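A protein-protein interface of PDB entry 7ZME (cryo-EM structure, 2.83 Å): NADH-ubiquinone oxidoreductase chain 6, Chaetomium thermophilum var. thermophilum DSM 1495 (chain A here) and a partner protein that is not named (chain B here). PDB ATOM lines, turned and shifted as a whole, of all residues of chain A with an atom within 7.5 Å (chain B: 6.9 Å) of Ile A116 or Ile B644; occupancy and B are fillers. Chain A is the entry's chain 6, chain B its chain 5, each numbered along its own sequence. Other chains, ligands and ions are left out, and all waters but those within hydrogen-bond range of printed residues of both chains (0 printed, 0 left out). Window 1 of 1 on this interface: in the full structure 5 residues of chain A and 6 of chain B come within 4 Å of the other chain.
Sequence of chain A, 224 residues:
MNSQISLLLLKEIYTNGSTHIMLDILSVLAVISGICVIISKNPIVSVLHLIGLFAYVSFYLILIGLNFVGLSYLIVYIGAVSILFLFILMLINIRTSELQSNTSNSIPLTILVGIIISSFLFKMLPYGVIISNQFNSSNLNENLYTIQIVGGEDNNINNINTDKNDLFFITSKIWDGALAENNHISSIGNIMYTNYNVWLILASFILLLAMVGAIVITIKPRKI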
ATOM      1  N   THR A 110       3.696  -2.261   9.299  1.00  0.00           N
ATOM      2  CA  THR A 110       3.545  -2.331   7.848  1.00  0.00           C
ATOM      3  C   THR A 110       2.920  -3.649   7.413  1.00  0.00           C
ATOM      4  O   THR A 110       2.011  -3.665   6.576  1.00  0.00           O
ATOM      5  CB  THR A 110       4.907  -2.147   7.177  1.00  0.00           C
ATOM      6  OG1 THR A 110       5.466  -0.883   7.559  1.00  0.00           O
ATOM      7  CG2 THR A 110       4.786  -2.231   5.662  1.00  0.00           C
ATOM      8  N   ILE A 111       3.393  -4.764   7.969  1.00  0.00           N
ATOM      9  CA  ILE A 111       2.844  -6.067   7.608  1.00  0.00           C
ATOM     10  C   ILE A 111       1.384  -6.162   8.029  1.00  0.00           C
ATOM     11  O   ILE A 111       0.524  -6.607   7.260  1.00  0.00           O
ATOM     12  CB  ILE A 111       3.686  -7.194   8.233  1.00  0.00           C
ATOM     13  CG1 ILE A 111       5.088  -7.215   7.621  1.00  0.00           C
ATOM     14  CG2 ILE A 111       3.002  -8.540   8.045  1.00  0.00           C
ATOM     15  CD1 ILE A 111       5.108  -7.587   6.156  1.00  0.00           C
ATOM     16  N   LEU A 112       1.083  -5.741   9.259  1.00  0.00           N
ATOM     17  CA  LEU A 112      -0.284  -5.831   9.763  1.00  0.00           C
ATOM     18  C   LEU A 112      -1.219  -4.905   8.995  1.00  0.00           C
ATOM     19  O   LEU A 112      -2.279  -5.331   8.522  1.00  0.00           O
ATOM     20  CB  LEU A 112      -0.311  -5.501  11.253  1.00  0.00           C
ATOM     21  CG  LEU A 112       0.054  -6.636  12.210  1.00  0.00           C
ATOM     22  CD1 LEU A 112      -0.133  -6.186  13.647  1.00  0.00           C
ATOM     23  CD2 LEU A 112      -0.773  -7.877  11.913  1.00  0.00           C
ATOM     24  N   VAL A 113      -0.844  -3.631   8.863  1.00  0.00           N
ATOM     25  CA  VAL A 113      -1.703  -2.672   8.174  1.00  0.00           C
ATOM     26  C   VAL A 113      -1.834  -3.036   6.703  1.00  0.00           C
ATOM     27  O   VAL A 113      -2.915  -2.920   6.113  1.00  0.00           O
ATOM     28  CB  VAL A 113      -1.162  -1.242   8.365  1.00  0.00           C
ATOM     29  CG1 VAL A 113      -1.789  -0.286   7.364  1.00  0.00           C
ATOM     30  CG2 VAL A 113      -1.424  -0.770   9.783  1.00  0.00           C
ATOM     31  N   GLY A 114      -0.742  -3.497   6.090  1.00  0.00           N
ATOM     32  CA  GLY A 114      -0.802  -3.865   4.686  1.00  0.00           C
ATOM     33  C   GLY A 114      -1.757  -5.012   4.423  1.00  0.00           C
ATOM     34  O   GLY A 114      -2.576  -4.956   3.504  1.00  0.00           O
ATOM     35  N   ILE A 115      -1.673  -6.066   5.234  1.00  0.00           N
ATOM     36  CA  ILE A 115      -2.499  -7.247   5.006  1.00  0.00           C
ATOM     37  C   ILE A 115      -3.967  -6.934   5.265  1.00  0.00           C
ATOM     38  O   ILE A 115      -4.842  -7.281   4.465  1.00  0.00           O
ATOM     39  CB  ILE A 115      -2.011  -8.415   5.881  1.00  0.00           C
ATOM     40  CG1 ILE A 115      -0.693  -8.970   5.341  1.00  0.00           C
ATOM     41  CG2 ILE A 115      -3.061  -9.513   5.947  1.00  0.00           C
ATOM     42  CD1 ILE A 115      -0.117 -10.087   6.178  1.00  0.00           C
ATOM     43  N   ILE A 116      -4.256  -6.268   6.383  1.00  0.00           N
ATOM     44  CA  ILE A 116      -5.644  -6.058   6.787  1.00  0.00           C
ATOM     45  C   ILE A 116      -6.371  -5.177   5.779  1.00  0.00           C
ATOM     46  O   ILE A 116      -7.462  -5.518   5.310  1.00  0.00           O
ATOM     47  CB  ILE A 116      -5.704  -5.463   8.205  1.00  0.00           C
ATOM     48  CG1 ILE A 116      -5.351  -6.532   9.241  1.00  0.00           C
ATOM     49  CG2 ILE A 116      -7.079  -4.881   8.481  1.00  0.00           C
ATOM     50  CD1 ILE A 116      -5.144  -5.987  10.635  1.00  0.00           C
ATOM     51  N   ILE A 117      -5.777  -4.037   5.424  1.00  0.00           N
ATOM     52  CA  ILE A 117      -6.444  -3.115   4.510  1.00  0.00           C
ATOM     53  C   ILE A 117      -6.597  -3.746   3.132  1.00  0.00           C
ATOM     54  O   ILE A 117      -7.681  -3.721   2.542  1.00  0.00           O
ATOM     55  CB  ILE A 117      -5.685  -1.778   4.439  1.00  0.00           C
ATOM     56  CG1 ILE A 117      -5.539  -1.167   5.829  1.00  0.00           C
ATOM     57  CG2 ILE A 117      -6.422  -0.801   3.568  1.00  0.00           C
ATOM     58  CD1 ILE A 117      -5.018   0.248   5.807  1.00  0.00           C
ATOM     59  N   SER A 118      -5.523  -4.343   2.612  1.00  0.00           N
ATOM     60  CA  SER A 118      -5.571  -4.912   1.268  1.00  0.00           C
ATOM     61  C   SER A 118      -6.581  -6.047   1.174  1.00  0.00           C
ATOM     62  O   SER A 118      -7.329  -6.140   0.195  1.00  0.00           O
ATOM     63  CB  SER A 118      -4.182  -5.398   0.857  1.00  0.00           C
ATOM     64  OG  SER A 118      -3.578  -6.138   1.901  1.00  0.00           O
ATOM     65  N   SER A 119      -6.607  -6.930   2.173  1.00  0.00           N
ATOM     66  CA  SER A 119      -7.595  -8.003   2.175  1.00  0.00           C
ATOM     67  C   SER A 119      -9.007  -7.447   2.290  1.00  0.00           C
ATOM     68  O   SER A 119      -9.921  -7.902   1.594  1.00  0.00           O
ATOM     69  CB  SER A 119      -7.306  -8.982   3.312  1.00  0.00           C
ATOM     70  OG  SER A 119      -8.463  -9.726   3.652  1.00  0.00           O
ATOM     71  N   PHE A 120      -9.199  -6.453   3.157  1.00  0.00           N
ATOM     72  CA  PHE A 120     -10.514  -5.842   3.307  1.00  0.00           C
ATOM     73  C   PHE A 120     -10.896  -5.009   2.094  1.00  0.00           C
ATOM     74  O   PHE A 120     -12.079  -4.941   1.742  1.00  0.00           O
ATOM     75  CB  PHE A 120     -10.552  -4.985   4.566  1.00  0.00           C
ATOM     76  CG  PHE A 120     -10.748  -5.773   5.818  1.00  0.00           C
ATOM     77  CD1 PHE A 120     -10.803  -7.155   5.777  1.00  0.00           C
ATOM     78  CD2 PHE A 120     -10.894  -5.137   7.030  1.00  0.00           C
ATOM     79  CE1 PHE A 120     -10.991  -7.886   6.928  1.00  0.00           C
ATOM     80  CE2 PHE A 120     -11.086  -5.860   8.182  1.00  0.00           C
ATOM     81  CZ  PHE A 120     -11.133  -7.236   8.135  1.00  0.00           C
ATOM     82  N   LEU A 121      -9.928  -4.373   1.449  1.00  0.00           N
ATOM     83  CA  LEU A 121     -10.222  -3.501   0.326  1.00  0.00           C
ATOM     84  C   LEU A 121     -10.244  -4.245  -1.004  1.00  0.00           C
ATOM     85  O   LEU A 121     -10.353  -3.606  -2.054  1.00  0.00           O
ATOM     86  CB  LEU A 121      -9.205  -2.358   0.252  1.00  0.00           C
ATOM     87  CG  LEU A 121      -9.358  -1.074   1.076  1.00  0.00           C
ATOM     88  CD1 LEU A 121      -8.243  -0.102   0.723  1.00  0.00           C
ATOM     89  CD2 LEU A 121     -10.703  -0.402   0.929  1.00  0.00           C
ATOM     90  N   PHE A 122     -10.130  -5.575  -0.990  1.00  0.00           N
ATOM     91  CA  PHE A 122     -10.117  -6.334  -2.235  1.00  0.00           C
ATOM     92  C   PHE A 122     -11.527  -6.600  -2.747  1.00  0.00           C
ATOM     93  O   PHE A 122     -11.835  -6.321  -3.909  1.00  0.00           O
ATOM     94  CB  PHE A 122      -9.365  -7.651  -2.046  1.00  0.00           C
ATOM     95  CG  PHE A 122      -8.755  -8.182  -3.310  1.00  0.00           C
ATOM     96  CD1 PHE A 122      -7.660  -7.561  -3.886  1.00  0.00           C
ATOM     97  CD2 PHE A 122      -9.293  -9.294  -3.935  1.00  0.00           C
ATOM     98  CE1 PHE A 122      -7.102  -8.051  -5.053  1.00  0.00           C
ATOM     99  CE2 PHE A 122      -8.742  -9.786  -5.102  1.00  0.00           C
ATOM    100  CZ  PHE A 122      -7.646  -9.164  -5.662  1.00  0.00           C
ATOM    101  N   PHE B 639      -9.330   3.646  11.933  1.00  0.00           N
ATOM    102  CA  PHE B 639      -9.933   3.321  10.646  1.00  0.00           C
ATOM    103  C   PHE B 639      -9.978   1.816  10.425  1.00  0.00           C
ATOM    104  O   PHE B 639     -11.035   1.251  10.124  1.00  0.00           O
ATOM    105  CB  PHE B 639      -9.156   4.018   9.527  1.00  0.00           C
ATOM    106  CG  PHE B 639      -9.521   3.554   8.149  1.00  0.00           C
ATOM    107  CD1 PHE B 639     -10.637   4.057   7.511  1.00  0.00           C
ATOM    108  CD2 PHE B 639      -8.736   2.628   7.485  1.00  0.00           C
ATOM    109  CE1 PHE B 639     -10.970   3.642   6.244  1.00  0.00           C
ATOM    110  CE2 PHE B 639      -9.066   2.208   6.223  1.00  0.00           C
ATOM    111  CZ  PHE B 639     -10.185   2.717   5.600  1.00  0.00           C
ATOM    112  N   ILE B 640      -8.836   1.145  10.580  1.00  0.00           N
ATOM    113  CA  ILE B 640      -8.782  -0.285  10.307  1.00  0.00           C
ATOM    114  C   ILE B 640      -9.562  -1.071  11.350  1.00  0.00           C
ATOM    115  O   ILE B 640     -10.113  -2.133  11.046  1.00  0.00           O
ATOM    116  CB  ILE B 640      -7.319  -0.756  10.217  1.00  0.00           C
ATOM    117  CG1 ILE B 640      -6.595  -0.538  11.542  1.00  0.00           C
ATOM    118  CG2 ILE B 640      -6.588  -0.021   9.117  1.00  0.00           C
ATOM    119  CD1 ILE B 640      -5.241  -1.183  11.590  1.00  0.00           C
ATOM    120  N   LEU B 641      -9.626  -0.572  12.587  1.00  0.00           N
ATOM    121  CA  LEU B 641     -10.383  -1.260  13.627  1.00  0.00           C
ATOM    122  C   LEU B 641     -11.874  -1.263  13.316  1.00  0.00           C
ATOM    123  O   LEU B 641     -12.568  -2.247  13.595  1.00  0.00           O
ATOM    124  CB  LEU B 641     -10.119  -0.611  14.983  1.00  0.00           C
ATOM    125  CG  LEU B 641      -9.045  -1.255  15.860  1.00  0.00           C
ATOM    126  CD1 LEU B 641      -8.836  -0.444  17.114  1.00  0.00           C
ATOM    127  CD2 LEU B 641      -9.399  -2.689  16.200  1.00  0.00           C
ATOM    128  N   TYR B 642     -12.386  -0.166  12.754  1.00  0.00           N
ATOM    129  CA  TYR B 642     -13.783  -0.133  12.330  1.00  0.00           C
ATOM    130  C   TYR B 642     -14.030  -1.101  11.183  1.00  0.00           C
ATOM    131  O   TYR B 642     -15.124  -1.665  11.067  1.00  0.00           O
ATOM    132  CB  TYR B 642     -14.184   1.284  11.925  1.00  0.00           C
ATOM    133  CG  TYR B 642     -14.588   2.177  13.074  1.00  0.00           C
ATOM    134  CD1 TYR B 642     -13.882   2.173  14.267  1.00  0.00           C
ATOM    135  CD2 TYR B 642     -15.665   3.035  12.959  1.00  0.00           C
ATOM    136  CE1 TYR B 642     -14.248   2.996  15.315  1.00  0.00           C
ATOM    137  CE2 TYR B 642     -16.036   3.860  13.998  1.00  0.00           C
ATOM    138  CZ  TYR B 642     -15.326   3.835  15.171  1.00  0.00           C
ATOM    139  OH  TYR B 642     -15.691   4.653  16.208  1.00  0.00           O
ATOM    140  N   LEU B 643     -13.036  -1.290  10.315  1.00  0.00           N
ATOM    141  CA  LEU B 643     -13.149  -2.310   9.278  1.00  0.00           C
ATOM    142  C   LEU B 643     -13.176  -3.707   9.885  1.00  0.00           C
ATOM    143  O   LEU B 643     -13.929  -4.572   9.428  1.00  0.00           O
ATOM    144  CB  LEU B 643     -12.003  -2.181   8.275  1.00  0.00           C
ATOM    145  CG  LEU B 643     -11.697  -0.829   7.624  1.00  0.00           C
ATOM    146  CD1 LEU B 643     -10.676  -1.009   6.526  1.00  0.00           C
ATOM    147  CD2 LEU B 643     -12.946  -0.183   7.067  1.00  0.00           C
ATOM    148  N   ILE B 644     -12.352  -3.950  10.908  1.00  0.00           N
ATOM    149  CA  ILE B 644     -12.354  -5.247  11.582  1.00  0.00           C
ATOM    150  C   ILE B 644     -13.733  -5.550  12.146  1.00  0.00           C
ATOM    151  O   ILE B 644     -14.289  -6.633  11.926  1.00  0.00           O
ATOM    152  CB  ILE B 644     -11.286  -5.288  12.691  1.00  0.00           C
ATOM    153  CG1 ILE B 644      -9.889  -5.043  12.130  1.00  0.00           C
ATOM    154  CG2 ILE B 644     -11.342  -6.608  13.438  1.00  0.00           C
ATOM    155  CD1 ILE B 644      -9.457  -6.065  11.130  1.00  0.00           C
ATOM    156  N   TYR B 645     -14.306  -4.598  12.882  1.00  0.00           N
ATOM    157  CA  TYR B 645     -15.582  -4.847  13.541  1.00  0.00           C
ATOM    158  C   TYR B 645     -16.690  -5.126  12.538  1.00  0.00           C
ATOM    159  O   TYR B 645     -17.531  -6.003  12.762  1.00  0.00           O
ATOM    160  CB  TYR B 645     -15.961  -3.669  14.429  1.00  0.00           C
ATOM    161  CG  TYR B 645     -17.196  -3.943  15.246  1.00  0.00           C
ATOM    162  CD1 TYR B 645     -17.217  -4.963  16.187  1.00  0.00           C
ATOM    163  CD2 TYR B 645     -18.357  -3.216  15.046  1.00  0.00           C
ATOM    164  CE1 TYR B 645     -18.351  -5.228  16.926  1.00  0.00           C
ATOM    165  CE2 TYR B 645     -19.490  -3.471  15.782  1.00  0.00           C
ATOM    166  CZ  TYR B 645     -19.481  -4.478  16.720  1.00  0.00           C
ATOM    167  OH  TYR B 645     -20.614  -4.734  17.450  1.00  0.00           O
ATOM    168  N   ASN B 646     -16.711  -4.392  11.429  1.00  0.00           N
ATOM    169  CA  ASN B 646     -17.824  -4.512  10.499  1.00  0.00           C
ATOM    170  C   ASN B 646     -17.648  -5.709   9.571  1.00  0.00           C
ATOM    171  O   ASN B 646     -18.557  -6.533   9.432  1.00  0.00           O
ATOM    172  CB  ASN B 646     -17.969  -3.219   9.696  1.00  0.00           C
ATOM    173  CG  ASN B 646     -19.261  -3.165   8.911  1.00  0.00           C
ATOM    174  OD1 ASN B 646     -20.060  -4.097   8.949  1.00  0.00           O
ATOM    175  ND2 ASN B 646     -19.474  -2.071   8.191  1.00  0.00           N
ATOM    176  N   ASN B 647     -16.482  -5.819   8.932  1.00  0.00           N
ATOM    177  CA  ASN B 647     -16.273  -6.869   7.941  1.00  0.00           C
ATOM    178  C   ASN B 647     -16.291  -8.255   8.574  1.00  0.00           C
ATOM    179  O   ASN B 647     -16.870  -9.192   8.012  1.00  0.00           O
ATOM    180  CB  ASN B 647     -14.957  -6.633   7.203  1.00  0.00           C
ATOM    181  CG  ASN B 647     -14.881  -7.385   5.890  1.00  0.00           C
ATOM    182  OD1 ASN B 647     -15.729  -8.226   5.590  1.00  0.00           O
ATOM    183  ND2 ASN B 647     -13.863  -7.080   5.096  1.00  0.00           N
ATOM    184  N   LEU B 648     -15.665  -8.409   9.739  1.00  0.00           N
ATOM    185  CA  LEU B 648     -15.540  -9.726  10.347  1.00  0.00           C
ATOM    186  C   LEU B 648     -16.799 -10.178  11.072  1.00  0.00           C
ATOM    187  O   LEU B 648     -16.847 -11.329  11.521  1.00  0.00           O
ATOM    188  CB  LEU B 648     -14.359  -9.750  11.319  1.00  0.00           C
ATOM    189  CG  LEU B 648     -12.971  -9.775  10.678  1.00  0.00           C
ATOM    190  CD1 LEU B 648     -11.888  -9.807  11.746  1.00  0.00           C
ATOM    191  CD2 LEU B 648     -12.840 -10.961   9.740  1.00  0.00           C
ATOM    192  N   LEU B 649     -17.810  -9.317  11.188  1.00  0.00           N
ATOM    193  CA  LEU B 649     -19.066  -9.653  11.859  1.00  0.00           C
ATOM    194  C   LEU B 649     -18.807 -10.149  13.281  1.00  0.00           C
ATOM    195  O   LEU B 649     -19.348 -11.163  13.729  1.00  0.00           O
ATOM    196  CB  LEU B 649     -19.861 -10.680  11.049  1.00  0.00           C
ATOM    197  CG  LEU B 649     -21.354 -10.816  11.359  1.00  0.00           C
ATOM    198  CD1 LEU B 649     -22.019  -9.451  11.430  1.00  0.00           C
ATOM    199  CD2 LEU B 649     -22.040 -11.702  10.330  1.00  0.00           C
ATOM    200  N   LEU B 650     -17.948  -9.424  13.990  1.00  0.00           N
ATOM    201  CA  LEU B 650     -17.619  -9.777  15.360  1.00  0.00           C
ATOM    202  C   LEU B 650     -18.841  -9.633  16.261  1.00  0.00           C
ATOM    203  O   LEU B 650     -19.806  -8.930  15.945  1.00  0.00           O
ATOM    204  CB  LEU B 650     -16.488  -8.893  15.884  1.00  0.00           C
ATOM    205  CG  LEU B 650     -15.215  -8.819  15.042  1.00  0.00           C
ATOM    206  CD1 LEU B 650     -14.244  -7.817  15.641  1.00  0.00           C
ATOM    207  CD2 LEU B 650     -14.571 -10.190  14.935  1.00  0.00           C
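Of the 13 printed residues of chain A, 3 touch a printed residue of chain B. Hydrophobic or aromatic side chains of chain A that line the printed part of chain B: Ile A116, Ile A117 and Phe A120. Of the 12 printed residues of chain B, 4 touch a printed residue of chain A. Hydrophobic or aromatic side chains of chain B that line the printed part of chain A: Ile B640, Leu B643 and Ile B644. Among the printed residues, no Asp or Glu carboxylate lies within 4 Å of a Lys or Arg side-chain nitrogen of the other chain.
Among the printed residues, pairs that only touch across the chains: Phe A120 with Asn B647 (3.1 Å), Phe A120 with Leu B643 (3.4 Å), Phe A120 with Ile B644 (3.4 Å), Ile A117 with Ile B640 (3.6 Å) and Ile A116 with Ile B644 (3.8 Å).
Ile A116 touches just one residue of chain B: Ile B644. Of chain A, only Ile A116 and Phe A120 come within 4 Å of Ile B644. Of the printed residues of chain A, Leu B643 touches Phe A120 (3.4 Å). Printed residues of chain B within 4 Å of Phe A120: Leu B643, Ile B644 and Asn B647. Printed residues of chain A within 4 Å of Ile B640: Ile A117. Of the printed residues of chain B, Ile A117 touches Ile B640 (3.6 Å). Of the printed residues of chain A, Asn B647 touches Phe A120 (3.1 Å). Ile A111 touches none of the printed residues of chain B. The nearest residue of chain B that does not touch Ile A116 is Ile B640 (4.5 Å).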
